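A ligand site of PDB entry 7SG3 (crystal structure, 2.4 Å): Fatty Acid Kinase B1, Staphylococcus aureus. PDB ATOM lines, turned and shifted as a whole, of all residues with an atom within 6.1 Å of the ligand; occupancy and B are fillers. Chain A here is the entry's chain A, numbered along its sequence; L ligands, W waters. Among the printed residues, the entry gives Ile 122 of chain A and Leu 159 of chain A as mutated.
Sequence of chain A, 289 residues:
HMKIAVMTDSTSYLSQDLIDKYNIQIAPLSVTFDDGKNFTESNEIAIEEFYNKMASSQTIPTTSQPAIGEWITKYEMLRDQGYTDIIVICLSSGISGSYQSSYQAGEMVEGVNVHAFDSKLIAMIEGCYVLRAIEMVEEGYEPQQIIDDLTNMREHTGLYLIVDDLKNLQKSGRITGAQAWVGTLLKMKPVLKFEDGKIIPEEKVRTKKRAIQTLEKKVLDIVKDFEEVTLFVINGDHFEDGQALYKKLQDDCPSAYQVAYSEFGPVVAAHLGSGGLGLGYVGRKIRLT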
ATOM      1  N   THR A  11      19.126  15.407 -19.999  1.00  0.00           N
ATOM      2  CA  THR A  11      18.216  15.277 -21.140  1.00  0.00           C
ATOM      3  C   THR A  11      17.566  16.593 -21.533  1.00  0.00           C
ATOM      4  O   THR A  11      16.865  16.635 -22.545  1.00  0.00           O
ATOM      5  CB  THR A  11      17.129  14.246 -20.840  1.00  0.00           C
ATOM      6  OG1 THR A  11      16.749  14.332 -19.467  1.00  0.00           O
ATOM      7  CG2 THR A  11      17.636  12.838 -21.140  1.00  0.00           C
ATOM      8  N   LEU A  29      22.291  11.639 -17.220  1.00  0.00           N
ATOM      9  CA  LEU A  29      21.829  10.289 -17.500  1.00  0.00           C
ATOM     10  C   LEU A  29      22.953   9.512 -18.173  1.00  0.00           C
ATOM     11  O   LEU A  29      24.031  10.036 -18.456  1.00  0.00           O
ATOM     12  CB  LEU A  29      20.569  10.331 -18.363  1.00  0.00           C
ATOM     13  CG  LEU A  29      19.272  10.699 -17.629  1.00  0.00           C
ATOM     14  CD1 LEU A  29      19.009  12.188 -17.703  1.00  0.00           C
ATOM     15  CD2 LEU A  29      18.077   9.914 -18.166  1.00  0.00           C
ATOM     16  N   SER A  30      22.709   8.223 -18.434  1.00  0.00           N
ATOM     17  CA  SER A  30      23.750   7.373 -18.995  1.00  0.00           C
ATOM     18  C   SER A  30      23.150   6.472 -20.064  1.00  0.00           C
ATOM     19  O   SER A  30      21.951   6.229 -20.112  1.00  0.00           O
ATOM     20  CB  SER A  30      24.425   6.532 -17.898  1.00  0.00           C
ATOM     21  OG  SER A  30      25.701   6.079 -18.325  1.00  0.00           O
ATOM     22  N   THR A  62      21.031   0.287 -23.540  1.00  0.00           N
ATOM     23  CA  THR A  62      20.086   0.596 -22.489  1.00  0.00           C
ATOM     24  C   THR A  62      20.383   1.984 -21.922  1.00  0.00           C
ATOM     25  O   THR A  62      21.529   2.441 -21.928  1.00  0.00           O
ATOM     26  CB  THR A  62      20.134  -0.435 -21.359  1.00  0.00           C
ATOM     27  OG1 THR A  62      21.434  -0.428 -20.750  1.00  0.00           O
ATOM     28  CG2 THR A  62      19.848  -1.829 -21.907  1.00  0.00           C
ATOM     29  N   THR A  63      19.344   2.650 -21.446  1.00  0.00           N
ATOM     30  CA  THR A  63      19.464   3.978 -20.857  1.00  0.00           C
ATOM     31  C   THR A  63      19.267   3.893 -19.351  1.00  0.00           C
ATOM     32  O   THR A  63      18.525   3.045 -18.849  1.00  0.00           O
ATOM     33  CB  THR A  63      18.455   4.940 -21.470  1.00  0.00           C
ATOM     34  OG1 THR A  63      17.168   4.305 -21.528  1.00  0.00           O
ATOM     35  CG2 THR A  63      18.877   5.335 -22.876  1.00  0.00           C
ATOM     36  N   SER A  64      19.935   4.792 -18.631  1.00  0.00           N
ATOM     37  CA  SER A  64      19.942   4.784 -17.179  1.00  0.00           C
ATOM     38  C   SER A  64      19.667   6.189 -16.652  1.00  0.00           C
ATOM     39  O   SER A  64      20.327   7.151 -17.064  1.00  0.00           O
ATOM     40  CB  SER A  64      21.270   4.271 -16.636  1.00  0.00           C
ATOM     41  OG  SER A  64      21.511   2.937 -17.048  1.00  0.00           O
ATOM     42  N   GLN A  65      18.688   6.292 -15.746  1.00  0.00           N
ATOM     43  CA  GLN A  65      18.393   7.533 -15.057  1.00  0.00           C
ATOM     44  C   GLN A  65      19.583   7.927 -14.175  1.00  0.00           C
ATOM     45  O   GLN A  65      20.434   7.094 -13.875  1.00  0.00           O
ATOM     46  CB  GLN A  65      17.140   7.378 -14.203  1.00  0.00           C
ATOM     47  CG  GLN A  65      17.366   6.546 -12.949  1.00  0.00           C
ATOM     48  CD  GLN A  65      16.148   5.750 -12.534  1.00  0.00           C
ATOM     49  OE1 GLN A  65      15.384   6.170 -11.664  1.00  0.00           O
ATOM     50  NE2 GLN A  65      15.962   4.593 -13.154  1.00  0.00           N
ATOM     51  N   LEU A  91      13.002  15.207 -17.163  1.00  0.00           N
ATOM     52  CA  LEU A  91      12.289  14.729 -18.335  1.00  0.00           C
ATOM     53  C   LEU A  91      11.024  13.999 -17.906  1.00  0.00           C
ATOM     54  O   LEU A  91      10.736  13.827 -16.718  1.00  0.00           O
ATOM     55  CB  LEU A  91      13.184  13.829 -19.172  1.00  0.00           C
ATOM     56  CG  LEU A  91      13.579  12.450 -18.616  1.00  0.00           C
ATOM     57  CD1 LEU A  91      13.918  11.509 -19.752  1.00  0.00           C
ATOM     58  CD2 LEU A  91      14.748  12.563 -17.657  1.00  0.00           C
ATOM     59  N   ILE A  95       8.343   8.299 -19.292  1.00  0.00           N
ATOM     60  CA  ILE A  95       9.349   7.651 -20.121  1.00  0.00           C
ATOM     61  C   ILE A  95      10.603   7.291 -19.349  1.00  0.00           C
ATOM     62  O   ILE A  95      11.389   6.449 -19.823  1.00  0.00           O
ATOM     63  CB  ILE A  95       9.702   8.528 -21.347  1.00  0.00           C
ATOM     64  CG1 ILE A  95      10.739   9.581 -20.979  1.00  0.00           C
ATOM     65  CG2 ILE A  95       8.454   9.170 -21.927  1.00  0.00           C
ATOM     66  CD1 ILE A  95      11.092  10.516 -22.119  1.00  0.00           C
ATOM     67  N   SER A  96      10.816   7.864 -18.168  1.00  0.00           N
ATOM     68  CA  SER A  96      12.038   7.624 -17.418  1.00  0.00           C
ATOM     69  C   SER A  96      11.727   7.752 -15.935  1.00  0.00           C
ATOM     70  O   SER A  96      10.712   8.327 -15.536  1.00  0.00           O
ATOM     71  CB  SER A  96      13.148   8.600 -17.832  1.00  0.00           C
ATOM     72  OG  SER A  96      14.238   8.560 -16.927  1.00  0.00           O
ATOM     73  N   GLY A  97      12.626   7.212 -15.118  1.00  0.00           N
ATOM     74  CA  GLY A  97      12.517   7.285 -13.677  1.00  0.00           C
ATOM     75  C   GLY A  97      13.309   8.411 -13.046  1.00  0.00           C
ATOM     76  O   GLY A  97      13.486   8.414 -11.828  1.00  0.00           O
ATOM     77  N   SER A  98      13.802   9.369 -13.841  1.00  0.00           N
ATOM     78  CA  SER A  98      14.645  10.420 -13.286  1.00  0.00           C
ATOM     79  C   SER A  98      13.853  11.348 -12.369  1.00  0.00           C
ATOM     80  O   SER A  98      14.383  11.799 -11.348  1.00  0.00           O
ATOM     81  CB  SER A  98      15.292  11.217 -14.428  1.00  0.00           C
ATOM     82  OG  SER A  98      15.856  12.428 -13.953  1.00  0.00           O
ATOM     83  N   ILE A 122      11.082  16.636 -23.135  1.00  0.00           N
ATOM     84  CA  ILE A 122      12.468  16.211 -23.314  1.00  0.00           C
ATOM     85  C   ILE A 122      13.182  17.279 -24.132  1.00  0.00           C
ATOM     86  O   ILE A 122      12.535  18.132 -24.752  1.00  0.00           O
ATOM     87  CB  ILE A 122      12.511  14.830 -24.007  1.00  0.00           C
ATOM     88  CG1 ILE A 122      13.915  14.228 -23.980  1.00  0.00           C
ATOM     89  CG2 ILE A 122      12.012  14.939 -25.422  1.00  0.00           C
ATOM     90  CD1 ILE A 122      14.150  13.263 -22.844  1.00  0.00           C
ATOM     91  N   ALA A 123      14.506  17.247 -24.095  1.00  0.00           N
ATOM     92  CA  ALA A 123      15.361  18.073 -24.957  1.00  0.00           C
ATOM     93  C   ALA A 123      15.151  19.543 -24.599  1.00  0.00           C
ATOM     94  O   ALA A 123      14.812  19.878 -23.452  1.00  0.00           O
ATOM     95  CB  ALA A 123      15.119  17.730 -26.413  1.00  0.00           C
ATOM     96  N   LEU A 159       5.599  18.212 -28.449  1.00  0.00           N
ATOM     97  CA  LEU A 159       6.723  17.810 -29.294  1.00  0.00           C
ATOM     98  C   LEU A 159       6.294  16.685 -30.217  1.00  0.00           C
ATOM     99  O   LEU A 159       5.867  15.618 -29.751  1.00  0.00           O
ATOM    100  CB  LEU A 159       7.910  17.374 -28.435  1.00  0.00           C
ATOM    101  CG  LEU A 159       9.034  16.656 -29.171  1.00  0.00           C
ATOM    102  CD1 LEU A 159       9.834  17.636 -30.032  1.00  0.00           C
ATOM    103  CD2 LEU A 159       9.945  15.959 -28.193  1.00  0.00           C
ATOM    104  N   LEU A 161       7.592  14.132 -33.505  1.00  0.00           N
ATOM    105  CA  LEU A 161       8.842  13.452 -33.788  1.00  0.00           C
ATOM    106  C   LEU A 161       8.718  12.570 -35.027  1.00  0.00           C
ATOM    107  O   LEU A 161       7.666  11.986 -35.282  1.00  0.00           O
ATOM    108  CB  LEU A 161       9.285  12.576 -32.614  1.00  0.00           C
ATOM    109  CG  LEU A 161       9.746  13.322 -31.359  1.00  0.00           C
ATOM    110  CD1 LEU A 161       9.625  12.421 -30.147  1.00  0.00           C
ATOM    111  CD2 LEU A 161      11.157  13.823 -31.559  1.00  0.00           C
ATOM    112  N   PHE A 194       4.274  13.665 -28.245  1.00  0.00           N
ATOM    113  CA  PHE A 194       4.195  13.616 -26.792  1.00  0.00           C
ATOM    114  C   PHE A 194       2.788  14.003 -26.356  1.00  0.00           C
ATOM    115  O   PHE A 194       2.226  14.988 -26.845  1.00  0.00           O
ATOM    116  CB  PHE A 194       5.221  14.544 -26.154  1.00  0.00           C
ATOM    117  CG  PHE A 194       6.537  13.875 -25.866  1.00  0.00           C
ATOM    118  CD1 PHE A 194       7.427  13.591 -26.893  1.00  0.00           C
ATOM    119  CD2 PHE A 194       6.898  13.544 -24.572  1.00  0.00           C
ATOM    120  CE1 PHE A 194       8.638  12.975 -26.635  1.00  0.00           C
ATOM    121  CE2 PHE A 194       8.111  12.930 -24.304  1.00  0.00           C
ATOM    122  CZ  PHE A 194       8.974  12.642 -25.344  1.00  0.00           C
ATOM    123  N   ILE A 199       4.880   8.868 -25.279  1.00  0.00           N
ATOM    124  CA  ILE A 199       5.136   8.906 -26.710  1.00  0.00           C
ATOM    125  C   ILE A 199       4.084   8.033 -27.391  1.00  0.00           C
ATOM    126  O   ILE A 199       4.061   6.815 -27.192  1.00  0.00           O
ATOM    127  CB  ILE A 199       6.553   8.443 -27.050  1.00  0.00           C
ATOM    128  CG1 ILE A 199       7.574   9.167 -26.153  1.00  0.00           C
ATOM    129  CG2 ILE A 199       6.870   8.705 -28.518  1.00  0.00           C
ATOM    130  CD1 ILE A 199       9.005   8.876 -26.507  1.00  0.00           C
ATOM    131  N   ILE A 234      14.654  20.112 -33.229  1.00  0.00           N
ATOM    132  CA  ILE A 234      15.555  19.235 -32.481  1.00  0.00           C
ATOM    133  C   ILE A 234      16.030  18.164 -33.445  1.00  0.00           C
ATOM    134  O   ILE A 234      15.309  17.207 -33.747  1.00  0.00           O
ATOM    135  CB  ILE A 234      14.868  18.624 -31.253  1.00  0.00           C
ATOM    136  CG1 ILE A 234      14.000  19.683 -30.569  1.00  0.00           C
ATOM    137  CG2 ILE A 234      15.904  18.107 -30.280  1.00  0.00           C
ATOM    138  CD1 ILE A 234      13.262  19.169 -29.353  1.00  0.00           C
ATOM    139  N   PHE A 264      19.571  16.753 -30.017  1.00  0.00           N
ATOM    140  CA  PHE A 264      19.496  15.916 -28.840  1.00  0.00           C
ATOM    141  C   PHE A 264      20.761  15.065 -28.706  1.00  0.00           C
ATOM    142  O   PHE A 264      21.576  14.957 -29.625  1.00  0.00           O
ATOM    143  CB  PHE A 264      18.246  15.023 -28.886  1.00  0.00           C
ATOM    144  CG  PHE A 264      17.904  14.537 -30.254  1.00  0.00           C
ATOM    145  CD1 PHE A 264      18.791  13.746 -30.980  1.00  0.00           C
ATOM    146  CD2 PHE A 264      16.689  14.861 -30.831  1.00  0.00           C
ATOM    147  CE1 PHE A 264      18.464  13.292 -32.232  1.00  0.00           C
ATOM    148  CE2 PHE A 264      16.363  14.419 -32.096  1.00  0.00           C
ATOM    149  CZ  PHE A 264      17.243  13.635 -32.799  1.00  0.00           C
ATOM    150  N   VAL A 267      21.223   9.825 -25.025  1.00  0.00           N
ATOM    151  CA  VAL A 267      20.097   9.095 -24.437  1.00  0.00           C
ATOM    152  C   VAL A 267      18.897   9.116 -25.368  1.00  0.00           C
ATOM    153  O   VAL A 267      18.198   8.113 -25.530  1.00  0.00           O
ATOM    154  CB  VAL A 267      19.755   9.683 -23.047  1.00  0.00           C
ATOM    155  CG1 VAL A 267      18.345   9.285 -22.632  1.00  0.00           C
ATOM    156  CG2 VAL A 267      20.760   9.193 -22.017  1.00  0.00           C
ATOM    157  N   VAL A 268      18.645  10.254 -26.020  1.00  0.00           N
ATOM    158  CA  VAL A 268      17.534  10.340 -26.968  1.00  0.00           C
ATOM    159  C   VAL A 268      17.861   9.567 -28.247  1.00  0.00           C
ATOM    160  O   VAL A 268      17.009   8.849 -28.784  1.00  0.00           O
ATOM    161  CB  VAL A 268      17.205  11.814 -27.285  1.00  0.00           C
ATOM    162  CG1 VAL A 268      16.456  11.911 -28.600  1.00  0.00           C
ATOM    163  CG2 VAL A 268      16.410  12.446 -26.146  1.00  0.00           C
ATOM    164  N   HIS A 271      17.266   5.686 -28.510  1.00  0.00           N
ATOM    165  CA  HIS A 271      15.920   5.192 -28.744  1.00  0.00           C
ATOM    166  C   HIS A 271      15.307   5.721 -30.028  1.00  0.00           C
ATOM    167  O   HIS A 271      14.403   5.076 -30.583  1.00  0.00           O
ATOM    168  CB  HIS A 271      15.013   5.570 -27.559  1.00  0.00           C
ATOM    169  CG  HIS A 271      15.241   4.727 -26.346  1.00  0.00           C
ATOM    170  ND1 HIS A 271      15.433   5.264 -25.089  1.00  0.00           N
ATOM    171  CD2 HIS A 271      15.324   3.387 -26.190  1.00  0.00           C
ATOM    172  CE1 HIS A 271      15.611   4.290 -24.220  1.00  0.00           C
ATOM    173  NE2 HIS A 271      15.551   3.139 -24.859  1.00  0.00           N
ATOM    174  N   LEU A 272      15.769   6.868 -30.529  1.00  0.00           N
ATOM    175  CA  LEU A 272      15.238   7.422 -31.757  1.00  0.00           C
ATOM    176  C   LEU A 272      15.934   6.883 -32.999  1.00  0.00           C
ATOM    177  O   LEU A 272      15.332   6.857 -34.082  1.00  0.00           O
ATOM    178  CB  LEU A 272      15.334   8.950 -31.715  1.00  0.00           C
ATOM    179  CG  LEU A 272      14.410   9.744 -32.643  1.00  0.00           C
ATOM    180  CD1 LEU A 272      12.970   9.492 -32.265  1.00  0.00           C
ATOM    181  CD2 LEU A 272      14.735  11.224 -32.534  1.00  0.00           C
ATOM    182  N   GLY A 278      12.732  16.175 -34.571  1.00  0.00           N
ATOM    183  CA  GLY A 278      11.551  16.602 -33.862  1.00  0.00           C
ATOM    184  C   GLY A 278      11.300  18.086 -34.003  1.00  0.00           C
ATOM    185  O   GLY A 278      12.211  18.882 -34.230  1.00  0.00           O
HETATM  186  C1  LIG L   1      16.062   5.900 -18.311  1.00  0.00           C
HETATM  187  O1  LIG L   1      16.199   4.701 -18.599  1.00  0.00           O
HETATM  188  O2  LIG L   1      15.403   6.312 -17.345  1.00  0.00           O
HETATM  189  C2  LIG L   1      16.715   6.932 -19.210  1.00  0.00           C
HETATM  190  C3  LIG L   1      15.751   7.666 -20.052  1.00  0.00           C
HETATM  191  C4  LIG L   1      14.542   6.824 -20.405  1.00  0.00           C
HETATM  192  C5  LIG L   1      14.463   6.462 -21.855  1.00  0.00           C
HETATM  193  C6  LIG L   1      14.994   7.525 -22.764  1.00  0.00           C
HETATM  194  C7  LIG L   1      13.943   8.495 -23.229  1.00  0.00           C
HETATM  195  C8  LIG L   1      12.666   7.823 -23.676  1.00  0.00           C
HETATM  196  C9  LIG L   1      12.325   8.086 -25.112  1.00  0.00           C
HETATM  197  C10 LIG L   1      13.411   8.804 -25.845  1.00  0.00           C
HETATM  198  C11 LIG L   1      12.993   9.439 -27.132  1.00  0.00           C
HETATM  199  C12 LIG L   1      12.848  10.939 -27.054  1.00  0.00           C
HETATM  200  C13 LIG L   1      12.810  11.628 -28.393  1.00  0.00           C
HETATM  201  C14 LIG L   1      12.656  13.122 -28.311  1.00  0.00           C
HETATM  202  C15 LIG L   1      13.605  13.911 -29.183  1.00  0.00           C
HETATM  203  C16 LIG L   1      13.634  15.385 -28.899  1.00  0.00           C
HETATM  204  O   HOH W   1      11.425   4.981 -23.107  1.00  0.00           O
HETATM  205  O   HOH W   2      16.008   4.305 -15.757  1.00  0.00           O
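The side-chain hydroxyl of Ser 96 sits at hydrogen-bond distance from an oxygen (O2) of the ligand (2.6 Å). The backbone carbonyl oxygen of Thr 63 sits close to an oxygen (O1) of the ligand, 2.9 Å away. An oxygen (O1) of the ligand is in hydrogen-bond range of the side-chain hydroxyl of Thr 63, at 3.1 Å.
OG of Ser 96 sits at hydrogen-bond distance from N of Ser 98 (3.2 Å). O of Gly 97 lies close to OE1 of Gln 65 (2.9 Å). The backbone carbonyl oxygen of Thr 11 sits at hydrogen-bond distance from the backbone NH of Ala 123, at 2.9 Å. The backbone carbonyl oxygen (O) of Ser 30 lies within hydrogen-bond range of the backbone NH (N) of Ser 64. The backbone NH of Phe 194 is in hydrogen-bond range of the backbone carbonyl oxygen of Leu 159 (2.9 Å). The backbone carbonyl oxygen of Ile 234 sits at hydrogen-bond distance from the backbone NH of Gly 278.
Leu 29 touches the ligand. Ser 64 touches the ligand (N to O1, 3.7 Å). Gln 65 touches the ligand. O of Ile 95 touches C4 of the ligand, 3.2 Å away. Gly 97 touches the ligand. Ile 122 touches the ligand (CG2 to C14, 3.5 Å). CB of Ala 123 touches C16 of the ligand, at 3.7 Å. Leu 159 touches the ligand. Leu 161 touches the ligand. Ile 199 touches the ligand (CD1 to C9, 3.7 Å). Ile 234 touches the ligand. Phe 264 touches the ligand (CD2 to C15, 3.6 Å). CG1 of Val 267 touches C6 of the ligand, 3.8 Å away. CG1 of Val 268 touches C15 of the ligand, 3.5 Å away. His 271 touches the ligand. Hydrophobic or aromatic side chains that line the ligand: Leu 29, Ile 95, Ile 122, Ala 123, Leu 159, Leu 161, Ile 199, Ile 234, Phe 264, Val 267, Val 268 and His 271.
Water W2 bridges the side-chain amide nitrogen (NE2) of Gln 65 (2.6 Å) and an oxygen (O2) of the ligand (2.6 Å).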
